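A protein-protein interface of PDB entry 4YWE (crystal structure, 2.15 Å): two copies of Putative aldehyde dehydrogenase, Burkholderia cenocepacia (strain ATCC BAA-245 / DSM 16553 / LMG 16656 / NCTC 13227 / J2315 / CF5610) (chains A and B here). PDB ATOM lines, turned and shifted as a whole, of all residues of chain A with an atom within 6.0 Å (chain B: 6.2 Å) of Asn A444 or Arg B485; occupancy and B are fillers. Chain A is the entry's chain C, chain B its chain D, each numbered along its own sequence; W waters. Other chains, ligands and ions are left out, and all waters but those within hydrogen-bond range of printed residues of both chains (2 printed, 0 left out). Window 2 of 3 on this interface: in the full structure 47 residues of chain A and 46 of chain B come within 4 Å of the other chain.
Printed residues of chain B that touch a printed residue of chain A: Tyr B139, Ala B483, Ile B484 and Arg B485.
Hydrophobic or aromatic side chains of chain A within 4 Å of the printed part of chain B: Phe A442 and Ile A443.
Among the printed residues, 8 pairs touch across the chains.
No position is printed for both chains.
Among the printed residues, merely in contact across the chains: Phe A442 with Ala B483, Ile A443 with Ile B484, Asn A444 with Arg B485, Asn A445 with Tyr B139 and Asn A445 with Arg B485.
Water W1 bridges NH1 of Arg B485 (2.4 Å) and O of Asn A444 (3.4 Å).
Water W2 lies within hydrogen-bond range of the backbone carbonyl oxygen of Arg B485 (2.6 Å) and the side-chain amide nitrogen of Asn A444 (2.6 Å).
Asp A270 touches none of the printed residues of chain B.
Thr A423 touches none of the printed residues of chain B.
Of the printed residues of chain B, Ile A443 touches Ala B483, Ile B484 and Arg B485.
Asn A444 touches one residue of chain B.
Of the printed residues of chain B, Asn A445 touches Tyr B139 (3.7 Å), Ala B483 (3.1 Å) and Arg B485 (3.8 Å).
Of the printed residues of chain A, Tyr B139 touches Asn A445.
Of the printed residues of chain A, Ala B483 touches Phe A442 (3.5 Å), Ile A443 (3.0 Å) and Asn A445 (3.1 Å).
Arg B485 touches just these residues of chain A: Ile A443, Asn A444 and Asn A445.
The nearest printed residue of chain A that does not touch Ala B483 is Asn A444 (5.6 Å).
The backbone carbonyl oxygen (O) of Ala B483 sits at hydrogen-bond distance from the side-chain amide nitrogen (ND2) of Asn A445.
The backbone NH of Ile A443 sits at hydrogen-bond distance from the backbone carbonyl oxygen of Ala B483, 3.0 Å away.
The backbone NH (N) of Arg B485 lies within hydrogen-bond range of the backbone carbonyl oxygen (O) of Ile A443 (3.2 Å).
The side-chain amide nitrogen of Gln A429 lies close to the side-chain amide nitrogen of Asn A444, 3.2 Å away.
The backbone carbonyl oxygen of Thr B140 lies within hydrogen-bond range of the backbone NH of Ile B484 (2.9 Å).
The side-chain amide nitrogen of Asn A445 is in hydrogen-bond range of the backbone carbonyl oxygen of Ile A443.
O of Thr A423 lies close to OD1 of Asn A444.
The backbone carbonyl oxygen (O) of Ile A421 lies within hydrogen-bond range of the backbone NH (N) of Asn A444 (2.8 Å).
The backbone NH (N) of Ile A421 sits at hydrogen-bond distance from the backbone carbonyl oxygen (O) of Phe A442.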
ATOM      1  N   ALA A 269     -20.726 -30.689  17.077  1.00  0.00           N
ATOM      2  CA  ALA A 269     -22.105 -30.728  16.603  1.00  0.00           C
ATOM      3  C   ALA A 269     -23.097 -31.046  17.718  1.00  0.00           C
ATOM      4  O   ALA A 269     -22.757 -31.700  18.705  1.00  0.00           O
ATOM      5  CB  ALA A 269     -22.245 -31.743  15.479  1.00  0.00           C
ATOM      6  N   ASP A 270     -24.326 -30.569  17.549  1.00  0.00           N
ATOM      7  CA  ASP A 270     -25.415 -30.893  18.462  1.00  0.00           C
ATOM      8  C   ASP A 270     -25.937 -32.284  18.129  1.00  0.00           C
ATOM      9  O   ASP A 270     -26.791 -32.442  17.255  1.00  0.00           O
ATOM     10  CB  ASP A 270     -26.534 -29.852  18.362  1.00  0.00           C
ATOM     11  CG  ASP A 270     -27.588 -30.007  19.448  1.00  0.00           C
ATOM     12  OD1 ASP A 270     -27.634 -31.067  20.109  1.00  0.00           O
ATOM     13  OD2 ASP A 270     -28.382 -29.062  19.640  1.00  0.00           O
ATOM     14  N   VAL A 277     -32.462 -36.941  12.993  1.00  0.00           N
ATOM     15  CA  VAL A 277     -32.429 -36.554  11.590  1.00  0.00           C
ATOM     16  C   VAL A 277     -31.582 -37.544  10.798  1.00  0.00           C
ATOM     17  O   VAL A 277     -31.959 -37.949   9.698  1.00  0.00           O
ATOM     18  CB  VAL A 277     -31.902 -35.120  11.419  1.00  0.00           C
ATOM     19  CG1 VAL A 277     -31.892 -34.735   9.949  1.00  0.00           C
ATOM     20  CG2 VAL A 277     -32.753 -34.147  12.217  1.00  0.00           C
ATOM     21  N   ILE A 421     -24.455 -31.082   6.686  1.00  0.00           N
ATOM     22  CA  ILE A 421     -23.355 -30.598   7.509  1.00  0.00           C
ATOM     23  C   ILE A 421     -23.839 -30.335   8.928  1.00  0.00           C
ATOM     24  O   ILE A 421     -24.710 -29.493   9.148  1.00  0.00           O
ATOM     25  CB  ILE A 421     -22.724 -29.328   6.914  1.00  0.00           C
ATOM     26  CG1 ILE A 421     -22.144 -29.611   5.528  1.00  0.00           C
ATOM     27  CG2 ILE A 421     -21.643 -28.790   7.836  1.00  0.00           C
ATOM     28  CD1 ILE A 421     -21.655 -28.368   4.815  1.00  0.00           C
ATOM     29  N   TRP A 422     -23.269 -31.052   9.890  1.00  0.00           N
ATOM     30  CA  TRP A 422     -23.635 -30.872  11.289  1.00  0.00           C
ATOM     31  C   TRP A 422     -22.456 -30.352  12.102  1.00  0.00           C
ATOM     32  O   TRP A 422     -21.519 -31.093  12.405  1.00  0.00           O
ATOM     33  CB  TRP A 422     -24.155 -32.181  11.881  1.00  0.00           C
ATOM     34  CG  TRP A 422     -25.397 -32.674  11.208  1.00  0.00           C
ATOM     35  CD1 TRP A 422     -25.468 -33.479  10.110  1.00  0.00           C
ATOM     36  CD2 TRP A 422     -26.747 -32.384  11.582  1.00  0.00           C
ATOM     37  NE1 TRP A 422     -26.781 -33.714   9.781  1.00  0.00           N
ATOM     38  CE2 TRP A 422     -27.586 -33.051  10.669  1.00  0.00           C
ATOM     39  CE3 TRP A 422     -27.329 -31.626  12.604  1.00  0.00           C
ATOM     40  CZ2 TRP A 422     -28.975 -32.984  10.744  1.00  0.00           C
ATOM     41  CZ3 TRP A 422     -28.709 -31.562  12.677  1.00  0.00           C
ATOM     42  CH2 TRP A 422     -29.516 -32.238  11.755  1.00  0.00           C
ATOM     43  N   THR A 423     -22.513 -29.069  12.444  1.00  0.00           N
ATOM     44  CA  THR A 423     -21.477 -28.416  13.233  1.00  0.00           C
ATOM     45  C   THR A 423     -21.986 -27.065  13.722  1.00  0.00           C
ATOM     46  O   THR A 423     -22.863 -26.466  13.101  1.00  0.00           O
ATOM     47  CB  THR A 423     -20.176 -28.220  12.424  1.00  0.00           C
ATOM     48  OG1 THR A 423     -19.201 -27.550  13.233  1.00  0.00           O
ATOM     49  CG2 THR A 423     -20.442 -27.400  11.172  1.00  0.00           C
ATOM     50  N   ARG A 424     -21.440 -26.590  14.837  1.00  0.00           N
ATOM     51  CA  ARG A 424     -21.852 -25.306  15.390  1.00  0.00           C
ATOM     52  C   ARG A 424     -21.010 -24.163  14.832  1.00  0.00           C
ATOM     53  O   ARG A 424     -21.428 -23.006  14.854  1.00  0.00           O
ATOM     54  CB  ARG A 424     -21.762 -25.321  16.919  1.00  0.00           C
ATOM     55  CG  ARG A 424     -22.832 -26.157  17.607  1.00  0.00           C
ATOM     56  CD  ARG A 424     -22.697 -26.074  19.121  1.00  0.00           C
ATOM     57  NE  ARG A 424     -23.731 -26.836  19.818  1.00  0.00           N
ATOM     58  CZ  ARG A 424     -23.573 -28.079  20.264  1.00  0.00           C
ATOM     59  NH1 ARG A 424     -22.419 -28.708  20.087  1.00  0.00           N
ATOM     60  NH2 ARG A 424     -24.568 -28.693  20.889  1.00  0.00           N
ATOM     61  N   GLN A 429     -19.254 -24.164   8.370  1.00  0.00           N
ATOM     62  CA  GLN A 429     -20.513 -24.449   7.684  1.00  0.00           C
ATOM     63  C   GLN A 429     -20.488 -23.982   6.233  1.00  0.00           C
ATOM     64  O   GLN A 429     -20.691 -24.774   5.314  1.00  0.00           O
ATOM     65  CB  GLN A 429     -21.684 -23.787   8.416  1.00  0.00           C
ATOM     66  CG  GLN A 429     -22.017 -24.405   9.761  1.00  0.00           C
ATOM     67  CD  GLN A 429     -22.975 -23.551  10.571  1.00  0.00           C
ATOM     68  OE1 GLN A 429     -23.364 -22.462  10.148  1.00  0.00           O
ATOM     69  NE2 GLN A 429     -23.361 -24.044  11.743  1.00  0.00           N
ATOM     70  N   PHE A 442     -27.448 -28.948   3.175  1.00  0.00           N
ATOM     71  CA  PHE A 442     -28.232 -28.606   4.356  1.00  0.00           C
ATOM     72  C   PHE A 442     -27.335 -28.441   5.579  1.00  0.00           C
ATOM     73  O   PHE A 442     -26.472 -29.279   5.852  1.00  0.00           O
ATOM     74  CB  PHE A 442     -29.304 -29.669   4.612  1.00  0.00           C
ATOM     75  CG  PHE A 442     -30.344 -29.748   3.529  1.00  0.00           C
ATOM     76  CD1 PHE A 442     -31.393 -28.844   3.491  1.00  0.00           C
ATOM     77  CD2 PHE A 442     -30.269 -30.720   2.546  1.00  0.00           C
ATOM     78  CE1 PHE A 442     -32.350 -28.908   2.494  1.00  0.00           C
ATOM     79  CE2 PHE A 442     -31.225 -30.790   1.545  1.00  0.00           C
ATOM     80  CZ  PHE A 442     -32.264 -29.882   1.520  1.00  0.00           C
ATOM     81  N   ILE A 443     -27.544 -27.348   6.307  1.00  0.00           N
ATOM     82  CA  ILE A 443     -26.722 -27.021   7.466  1.00  0.00           C
ATOM     83  C   ILE A 443     -27.521 -27.190   8.754  1.00  0.00           C
ATOM     84  O   ILE A 443     -28.509 -26.490   8.980  1.00  0.00           O
ATOM     85  CB  ILE A 443     -26.156 -25.595   7.350  1.00  0.00           C
ATOM     86  CG1 ILE A 443     -25.181 -25.510   6.171  1.00  0.00           C
ATOM     87  CG2 ILE A 443     -25.467 -25.186   8.640  1.00  0.00           C
ATOM     88  CD1 ILE A 443     -24.570 -24.139   5.976  1.00  0.00           C
ATOM     89  N   ASN A 444     -27.079 -28.129   9.586  1.00  0.00           N
ATOM     90  CA  ASN A 444     -27.747 -28.471  10.842  1.00  0.00           C
ATOM     91  C   ASN A 444     -29.206 -28.867  10.617  1.00  0.00           C
ATOM     92  O   ASN A 444     -30.067 -28.639  11.469  1.00  0.00           O
ATOM     93  CB  ASN A 444     -27.647 -27.315  11.839  1.00  0.00           C
ATOM     94  CG  ASN A 444     -26.219 -27.052  12.277  1.00  0.00           C
ATOM     95  OD1 ASN A 444     -25.392 -27.965  12.316  1.00  0.00           O
ATOM     96  ND2 ASN A 444     -25.922 -25.803  12.615  1.00  0.00           N
ATOM     97  N   ASN A 445     -29.464 -29.456   9.455  1.00  0.00           N
ATOM     98  CA  ASN A 445     -30.737 -30.094   9.147  1.00  0.00           C
ATOM     99  C   ASN A 445     -30.512 -30.991   7.936  1.00  0.00           C
ATOM    100  O   ASN A 445     -29.378 -31.150   7.485  1.00  0.00           O
ATOM    101  CB  ASN A 445     -31.837 -29.066   8.874  1.00  0.00           C
ATOM    102  CG  ASN A 445     -31.682 -28.386   7.529  1.00  0.00           C
ATOM    103  OD1 ASN A 445     -32.452 -28.640   6.604  1.00  0.00           O
ATOM    104  ND2 ASN A 445     -30.691 -27.511   7.417  1.00  0.00           N
ATOM    105  N   TYR A 446     -31.581 -31.579   7.409  1.00  0.00           N
ATOM    106  CA  TYR A 446     -31.453 -32.429   6.231  1.00  0.00           C
ATOM    107  C   TYR A 446     -32.784 -32.591   5.507  1.00  0.00           C
ATOM    108  O   TYR A 446     -33.658 -33.332   5.954  1.00  0.00           O
ATOM    109  CB  TYR A 446     -30.899 -33.800   6.617  1.00  0.00           C
ATOM    110  CG  TYR A 446     -30.418 -34.615   5.441  1.00  0.00           C
ATOM    111  CD1 TYR A 446     -29.130 -34.457   4.946  1.00  0.00           C
ATOM    112  CD2 TYR A 446     -31.249 -35.538   4.823  1.00  0.00           C
ATOM    113  CE1 TYR A 446     -28.683 -35.198   3.873  1.00  0.00           C
ATOM    114  CE2 TYR A 446     -30.809 -36.285   3.750  1.00  0.00           C
ATOM    115  CZ  TYR A 446     -29.527 -36.110   3.280  1.00  0.00           C
ATOM    116  OH  TYR A 446     -29.084 -36.850   2.211  1.00  0.00           O
ATOM    117  N   GLY B 138     -37.037 -19.683  10.937  1.00  0.00           N
ATOM    118  CA  GLY B 138     -35.798 -20.207  11.480  1.00  0.00           C
ATOM    119  C   GLY B 138     -34.852 -20.722  10.412  1.00  0.00           C
ATOM    120  O   GLY B 138     -33.830 -21.337  10.717  1.00  0.00           O
ATOM    121  N   TYR B 139     -35.194 -20.468   9.153  1.00  0.00           N
ATOM    122  CA  TYR B 139     -34.371 -20.907   8.031  1.00  0.00           C
ATOM    123  C   TYR B 139     -33.881 -19.743   7.179  1.00  0.00           C
ATOM    124  O   TYR B 139     -34.525 -18.697   7.099  1.00  0.00           O
ATOM    125  CB  TYR B 139     -35.146 -21.884   7.144  1.00  0.00           C
ATOM    126  CG  TYR B 139     -35.169 -23.308   7.644  1.00  0.00           C
ATOM    127  CD1 TYR B 139     -36.095 -23.719   8.593  1.00  0.00           C
ATOM    128  CD2 TYR B 139     -34.271 -24.248   7.155  1.00  0.00           C
ATOM    129  CE1 TYR B 139     -36.121 -25.024   9.046  1.00  0.00           C
ATOM    130  CE2 TYR B 139     -34.289 -25.554   7.601  1.00  0.00           C
ATOM    131  CZ  TYR B 139     -35.216 -25.937   8.547  1.00  0.00           C
ATOM    132  OH  TYR B 139     -35.235 -27.237   8.994  1.00  0.00           O
ATOM    133  N   THR B 140     -32.731 -19.942   6.542  1.00  0.00           N
ATOM    134  CA  THR B 140     -32.222 -19.020   5.535  1.00  0.00           C
ATOM    135  C   THR B 140     -31.744 -19.832   4.336  1.00  0.00           C
ATOM    136  O   THR B 140     -30.835 -20.653   4.457  1.00  0.00           O
ATOM    137  CB  THR B 140     -31.072 -18.148   6.074  1.00  0.00           C
ATOM    138  OG1 THR B 140     -31.560 -17.298   7.120  1.00  0.00           O
ATOM    139  CG2 THR B 140     -30.492 -17.285   4.963  1.00  0.00           C
ATOM    140  N   ALA B 483     -29.454 -24.624   2.419  1.00  0.00           N
ATOM    141  CA  ALA B 483     -30.523 -24.368   3.378  1.00  0.00           C
ATOM    142  C   ALA B 483     -29.991 -24.428   4.805  1.00  0.00           C
ATOM    143  O   ALA B 483     -29.606 -25.492   5.295  1.00  0.00           O
ATOM    144  CB  ALA B 483     -31.660 -25.359   3.188  1.00  0.00           C
ATOM    145  N   ILE B 484     -29.974 -23.277   5.468  1.00  0.00           N
ATOM    146  CA  ILE B 484     -29.419 -23.167   6.810  1.00  0.00           C
ATOM    147  C   ILE B 484     -30.528 -23.113   7.853  1.00  0.00           C
ATOM    148  O   ILE B 484     -31.414 -22.264   7.777  1.00  0.00           O
ATOM    149  CB  ILE B 484     -28.516 -21.927   6.932  1.00  0.00           C
ATOM    150  CG1 ILE B 484     -27.528 -21.861   5.765  1.00  0.00           C
ATOM    151  CG2 ILE B 484     -27.787 -21.926   8.264  1.00  0.00           C
ATOM    152  CD1 ILE B 484     -26.743 -20.568   5.708  1.00  0.00           C
ATOM    153  N   ARG B 485     -30.478 -24.017   8.827  1.00  0.00           N
ATOM    154  CA  ARG B 485     -31.396 -23.954   9.958  1.00  0.00           C
ATOM    155  C   ARG B 485     -30.696 -23.309  11.147  1.00  0.00           C
ATOM    156  O   ARG B 485     -29.736 -23.859  11.689  1.00  0.00           O
ATOM    157  CB  ARG B 485     -31.915 -25.342  10.336  1.00  0.00           C
ATOM    158  CG  ARG B 485     -32.936 -25.315  11.467  1.00  0.00           C
ATOM    159  CD  ARG B 485     -33.468 -26.700  11.792  1.00  0.00           C
ATOM    160  NE  ARG B 485     -34.436 -26.664  12.885  1.00  0.00           N
ATOM    161  CZ  ARG B 485     -35.019 -27.739  13.405  1.00  0.00           C
ATOM    162  NH1 ARG B 485     -34.734 -28.945  12.933  1.00  0.00           N
ATOM    163  NH2 ARG B 485     -35.889 -27.609  14.400  1.00  0.00           N
ATOM    164  N   HIS B 486     -31.183 -22.140  11.548  1.00  0.00           N
ATOM    165  CA  HIS B 486     -30.539 -21.363  12.600  1.00  0.00           C
ATOM    166  C   HIS B 486     -31.520 -20.979  13.702  1.00  0.00           C
ATOM    167  O   HIS B 486     -31.121 -20.465  14.746  1.00  0.00           O
ATOM    168  CB  HIS B 486     -29.896 -20.107  12.007  1.00  0.00           C
ATOM    169  CG  HIS B 486     -30.816 -19.313  11.134  1.00  0.00           C
ATOM    170  ND1 HIS B 486     -31.861 -18.566  11.637  1.00  0.00           N
ATOM    171  CD2 HIS B 486     -30.856 -19.156   9.789  1.00  0.00           C
ATOM    172  CE1 HIS B 486     -32.499 -17.980  10.641  1.00  0.00           C
ATOM    173  NE2 HIS B 486     -31.910 -18.321   9.509  1.00  0.00           N
ATOM    174  N   GLY B 487     -32.804 -21.230  13.464  1.00  0.00           N
ATOM    175  CA  GLY B 487     -33.830 -20.924  14.445  1.00  0.00           C
ATOM    176  C   GLY B 487     -34.111 -19.442  14.587  1.00  0.00           C
ATOM    177  O   GLY B 487     -34.933 -19.030  15.404  1.00  0.00           O
ATOM    178  OXT GLY B 487     -33.522 -18.611  13.894  1.00  0.00           O
HETATM  179  O   HOH W   1     -32.857 -30.310  12.315  1.00  0.00           O
HETATM  180  O   HOH W   2     -27.213 -23.619  12.135  1.00  0.00           O
